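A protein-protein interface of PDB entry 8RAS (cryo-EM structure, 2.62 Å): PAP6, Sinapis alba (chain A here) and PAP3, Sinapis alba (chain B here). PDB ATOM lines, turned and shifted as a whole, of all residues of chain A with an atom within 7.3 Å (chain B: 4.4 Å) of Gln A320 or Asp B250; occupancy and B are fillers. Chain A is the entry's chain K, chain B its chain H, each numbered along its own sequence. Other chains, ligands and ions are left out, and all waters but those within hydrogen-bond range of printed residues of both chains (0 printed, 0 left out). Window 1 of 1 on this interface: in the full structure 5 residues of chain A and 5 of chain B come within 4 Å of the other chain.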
ATOM      1  N   TYR A 317      13.215  39.677   2.962  1.00  0.00           N
ATOM      2  CA  TYR A 317      13.880  38.402   2.735  1.00  0.00           C
ATOM      3  C   TYR A 317      14.682  38.428   1.439  1.00  0.00           C
ATOM      4  O   TYR A 317      14.224  38.940   0.414  1.00  0.00           O
ATOM      5  CB  TYR A 317      12.855  37.269   2.700  1.00  0.00           C
ATOM      6  CG  TYR A 317      13.408  35.944   2.226  1.00  0.00           C
ATOM      7  CD1 TYR A 317      13.322  35.567   0.892  1.00  0.00           C
ATOM      8  CD2 TYR A 317      14.022  35.072   3.114  1.00  0.00           C
ATOM      9  CE1 TYR A 317      13.827  34.360   0.459  1.00  0.00           C
ATOM     10  CE2 TYR A 317      14.531  33.863   2.687  1.00  0.00           C
ATOM     11  CZ  TYR A 317      14.432  33.512   1.360  1.00  0.00           C
ATOM     12  OH  TYR A 317      14.937  32.308   0.931  1.00  0.00           O
ATOM     13  N   THR A 318      15.892  37.866   1.494  1.00  0.00           N
ATOM     14  CA  THR A 318      16.775  37.759   0.343  1.00  0.00           C
ATOM     15  C   THR A 318      17.398  36.368   0.372  1.00  0.00           C
ATOM     16  O   THR A 318      17.948  35.961   1.412  1.00  0.00           O
ATOM     17  CB  THR A 318      17.865  38.833   0.355  1.00  0.00           C
ATOM     18  OG1 THR A 318      17.261  40.130   0.383  1.00  0.00           O
ATOM     19  CG2 THR A 318      18.741  38.718  -0.881  1.00  0.00           C
ATOM     20  N   PRO A 319      17.324  35.613  -0.724  1.00  0.00           N
ATOM     21  CA  PRO A 319      17.920  34.274  -0.735  1.00  0.00           C
ATOM     22  C   PRO A 319      19.431  34.333  -0.577  1.00  0.00           C
ATOM     23  O   PRO A 319      20.093  35.270  -1.027  1.00  0.00           O
ATOM     24  CB  PRO A 319      17.518  33.714  -2.104  1.00  0.00           C
ATOM     25  CG  PRO A 319      17.225  34.903  -2.928  1.00  0.00           C
ATOM     26  CD  PRO A 319      16.673  35.939  -2.002  1.00  0.00           C
ATOM     27  N   GLN A 320      19.974  33.306   0.078  1.00  0.00           N
ATOM     28  CA  GLN A 320      21.386  33.311   0.439  1.00  0.00           C
ATOM     29  C   GLN A 320      22.290  33.004  -0.749  1.00  0.00           C
ATOM     30  O   GLN A 320      23.375  33.585  -0.868  1.00  0.00           O
ATOM     31  CB  GLN A 320      21.635  32.308   1.565  1.00  0.00           C
ATOM     32  CG  GLN A 320      22.840  32.628   2.425  1.00  0.00           C
ATOM     33  CD  GLN A 320      22.948  31.720   3.628  1.00  0.00           C
ATOM     34  OE1 GLN A 320      21.995  31.031   3.986  1.00  0.00           O
ATOM     35  NE2 GLN A 320      24.116  31.708   4.258  1.00  0.00           N
ATOM     36  N   TYR A 321      21.872  32.105  -1.637  1.00  0.00           N
ATOM     37  CA  TYR A 321      22.761  31.590  -2.670  1.00  0.00           C
ATOM     38  C   TYR A 321      22.324  31.956  -4.079  1.00  0.00           C
ATOM     39  O   TYR A 321      23.124  32.510  -4.843  1.00  0.00           O
ATOM     40  CB  TYR A 321      22.882  30.066  -2.530  1.00  0.00           C
ATOM     41  CG  TYR A 321      23.344  29.635  -1.159  1.00  0.00           C
ATOM     42  CD1 TYR A 321      24.669  29.790  -0.773  1.00  0.00           C
ATOM     43  CD2 TYR A 321      22.456  29.091  -0.244  1.00  0.00           C
ATOM     44  CE1 TYR A 321      25.095  29.405   0.478  1.00  0.00           C
ATOM     45  CE2 TYR A 321      22.874  28.705   1.010  1.00  0.00           C
ATOM     46  CZ  TYR A 321      24.194  28.863   1.365  1.00  0.00           C
ATOM     47  OH  TYR A 321      24.614  28.477   2.615  1.00  0.00           O
ATOM     48  N   PHE A 322      21.084  31.659  -4.457  1.00  0.00           N
ATOM     49  CA  PHE A 322      20.617  31.976  -5.797  1.00  0.00           C
ATOM     50  C   PHE A 322      19.117  32.216  -5.761  1.00  0.00           C
ATOM     51  O   PHE A 322      18.409  31.727  -4.878  1.00  0.00           O
ATOM     52  CB  PHE A 322      20.959  30.866  -6.799  1.00  0.00           C
ATOM     53  CG  PHE A 322      20.645  29.482  -6.308  1.00  0.00           C
ATOM     54  CD1 PHE A 322      19.385  28.939  -6.488  1.00  0.00           C
ATOM     55  CD2 PHE A 322      21.610  28.723  -5.671  1.00  0.00           C
ATOM     56  CE1 PHE A 322      19.092  27.670  -6.039  1.00  0.00           C
ATOM     57  CE2 PHE A 322      21.322  27.451  -5.219  1.00  0.00           C
ATOM     58  CZ  PHE A 322      20.061  26.925  -5.404  1.00  0.00           C
ATOM     59  N   ALA A 323      18.641  32.979  -6.740  1.00  0.00           N
ATOM     60  CA  ALA A 323      17.222  33.274  -6.843  1.00  0.00           C
ATOM     61  C   ALA A 323      16.456  32.067  -7.369  1.00  0.00           C
ATOM     62  O   ALA A 323      17.000  31.213  -8.072  1.00  0.00           O
ATOM     63  CB  ALA A 323      16.989  34.475  -7.756  1.00  0.00           C
ATOM     64  N   ASP B 248      21.549  28.908   9.558  1.00  0.00           N
ATOM     65  CA  ASP B 248      21.522  28.766   8.106  1.00  0.00           C
ATOM     66  C   ASP B 248      20.147  29.183   7.601  1.00  0.00           C
ATOM     67  O   ASP B 248      19.169  28.446   7.768  1.00  0.00           O
ATOM     68  CB  ASP B 248      21.852  27.334   7.693  1.00  0.00           C
ATOM     69  CG  ASP B 248      23.194  26.870   8.221  1.00  0.00           C
ATOM     70  OD1 ASP B 248      24.115  27.707   8.318  1.00  0.00           O
ATOM     71  OD2 ASP B 248      23.328  25.671   8.539  1.00  0.00           O
ATOM     72  N   GLN B 249      20.075  30.364   6.984  1.00  0.00           N
ATOM     73  CA  GLN B 249      18.797  30.877   6.497  1.00  0.00           C
ATOM     74  C   GLN B 249      18.221  29.984   5.406  1.00  0.00           C
ATOM     75  O   GLN B 249      17.027  29.666   5.414  1.00  0.00           O
ATOM     76  CB  GLN B 249      18.970  32.306   5.986  1.00  0.00           C
ATOM     77  CG  GLN B 249      17.719  32.892   5.362  1.00  0.00           C
ATOM     78  CD  GLN B 249      18.026  33.889   4.267  1.00  0.00           C
ATOM     79  OE1 GLN B 249      18.308  33.511   3.131  1.00  0.00           O
ATOM     80  NE2 GLN B 249      17.973  35.171   4.602  1.00  0.00           N
ATOM     81  N   ASP B 250      19.055  29.567   4.460  1.00  0.00           N
ATOM     82  CA  ASP B 250      18.623  28.764   3.328  1.00  0.00           C
ATOM     83  C   ASP B 250      19.382  27.445   3.305  1.00  0.00           C
ATOM     84  O   ASP B 250      20.493  27.333   3.827  1.00  0.00           O
ATOM     85  CB  ASP B 250      18.834  29.508   2.004  1.00  0.00           C
ATOM     86  CG  ASP B 250      17.719  30.485   1.701  1.00  0.00           C
ATOM     87  OD1 ASP B 250      16.571  30.232   2.125  1.00  0.00           O
ATOM     88  OD2 ASP B 250      17.989  31.505   1.037  1.00  0.00           O
ATOM     89  N   PHE B 251      18.766  26.441   2.689  1.00  0.00           N
ATOM     90  CA  PHE B 251      19.388  25.134   2.558  1.00  0.00           C
ATOM     91  C   PHE B 251      20.272  25.085   1.322  1.00  0.00           C
ATOM     92  O   PHE B 251      19.896  25.568   0.250  1.00  0.00           O
ATOM     93  CB  PHE B 251      18.339  24.024   2.483  1.00  0.00           C
ATOM     94  CG  PHE B 251      18.925  22.666   2.224  1.00  0.00           C
ATOM     95  CD1 PHE B 251      19.497  21.939   3.252  1.00  0.00           C
ATOM     96  CD2 PHE B 251      18.915  22.122   0.950  1.00  0.00           C
ATOM     97  CE1 PHE B 251      20.043  20.694   3.017  1.00  0.00           C
ATOM     98  CE2 PHE B 251      19.461  20.878   0.710  1.00  0.00           C
ATOM     99  CZ  PHE B 251      20.025  20.162   1.746  1.00  0.00           C
ATOM    100  N   TYR B 252      21.450  24.495   1.483  1.00  0.00           N
ATOM    101  CA  TYR B 252      22.406  24.275   0.415  1.00  0.00           C
ATOM    102  C   TYR B 252      23.000  22.886   0.597  1.00  0.00           C
ATOM    103  O   TYR B 252      23.035  22.375   1.722  1.00  0.00           O
ATOM    104  CB  TYR B 252      23.520  25.334   0.439  1.00  0.00           C
ATOM    105  CG  TYR B 252      24.323  25.429  -0.833  1.00  0.00           C
ATOM    106  CD1 TYR B 252      23.813  26.074  -1.950  1.00  0.00           C
ATOM    107  CD2 TYR B 252      25.593  24.881  -0.916  1.00  0.00           C
ATOM    108  CE1 TYR B 252      24.544  26.164  -3.113  1.00  0.00           C
ATOM    109  CE2 TYR B 252      26.331  24.965  -2.073  1.00  0.00           C
ATOM    110  CZ  TYR B 252      25.801  25.607  -3.168  1.00  0.00           C
ATOM    111  OH  TYR B 252      26.536  25.694  -4.323  1.00  0.00           O
ATOM    112  N   ARG B 258      16.900  19.418   6.897  1.00  0.00           N
ATOM    113  CA  ARG B 258      15.935  19.747   7.935  1.00  0.00           C
ATOM    114  C   ARG B 258      14.532  19.808   7.340  1.00  0.00           C
ATOM    115  O   ARG B 258      14.324  19.582   6.146  1.00  0.00           O
ATOM    116  CB  ARG B 258      16.301  21.075   8.603  1.00  0.00           C
ATOM    117  CG  ARG B 258      16.164  22.273   7.680  1.00  0.00           C
ATOM    118  CD  ARG B 258      17.232  23.321   7.940  1.00  0.00           C
ATOM    119  NE  ARG B 258      17.047  24.492   7.092  1.00  0.00           N
ATOM    120  CZ  ARG B 258      17.787  25.591   7.155  1.00  0.00           C
ATOM    121  NH1 ARG B 258      18.781  25.705   8.019  1.00  0.00           N
ATOM    122  NH2 ARG B 258      17.522  26.599   6.330  1.00  0.00           N
ATOM    123  N   PHE B 363      32.354  29.865   6.240  1.00  0.00           N
ATOM    124  CA  PHE B 363      31.342  30.900   6.378  1.00  0.00           C
ATOM    125  C   PHE B 363      31.931  32.127   7.058  1.00  0.00           C
ATOM    126  O   PHE B 363      32.885  32.034   7.835  1.00  0.00           O
ATOM    127  CB  PHE B 363      30.151  30.399   7.195  1.00  0.00           C
ATOM    128  CG  PHE B 363      29.236  29.478   6.448  1.00  0.00           C
ATOM    129  CD1 PHE B 363      28.357  29.971   5.503  1.00  0.00           C
ATOM    130  CD2 PHE B 363      29.239  28.121   6.707  1.00  0.00           C
ATOM    131  CE1 PHE B 363      27.510  29.126   4.820  1.00  0.00           C
ATOM    132  CE2 PHE B 363      28.393  27.273   6.030  1.00  0.00           C
ATOM    133  CZ  PHE B 363      27.527  27.776   5.085  1.00  0.00           C
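O of Thr A318 sits close to OE1 of Gln B249 (3.0 Å). OE1 of Gln B249 lies within hydrogen-bond range of N of Gln A320. N of Gln A320 lies within hydrogen-bond range of OD2 of Asp B250 (2.8 Å). OH of Tyr A317 lies within hydrogen-bond range of OD1 of Asp B250.
The backbone carbonyl oxygen of Gln B249 is in hydrogen-bond range of the guanidinium group of Arg B258 (3.2 Å). OE1 of Gln B249 lies close to OD2 of Asp B250, at 2.9 Å.
OE1 of Gln B249 touches CE2 of Tyr A317, at 3.8 Å. OE1 of Gln B249 touches CA of Pro A319, at 3.96 Å. Pro A319 touches Asp B250 (CA to OD2, 3.3 Å). Tyr A321 touches Asp B250. Tyr B252 touches Tyr A321 (CB to CE2, 3.5 Å). Tyr A321 touches Phe B363.
Asp B250 touches just these residues of chain A: Tyr A317 (2.9 Å), Pro A319 (3.3 Å), Gln A320 (2.8 Å) and Tyr A321 (3.9 Å). Of the printed residues of chain B, Thr A318 touches Gln B249 (3.0 Å). Of the printed residues of chain A, Tyr B252 touches Tyr A321. Of the printed residues of chain A, Gln B249 touches Tyr A317, Thr A318, Pro A319 and Gln A320. Of the printed residues of chain A, Phe B363 touches Tyr A321. Of the printed residues of chain B, Tyr A317 touches Gln B249 (3.8 Å) and Asp B250 (2.9 Å). Phe B251 touches none of the printed residues of chain A. Ala A323 touches none of the printed residues of chain B. The nearest residue of chain B that does not touch Gln A320 is Phe B363 (4.3 Å).
Hydrophobic or aromatic side chains of chain A within 4 Å of the printed part of chain B: Tyr A317, Pro A319 and Tyr A321.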
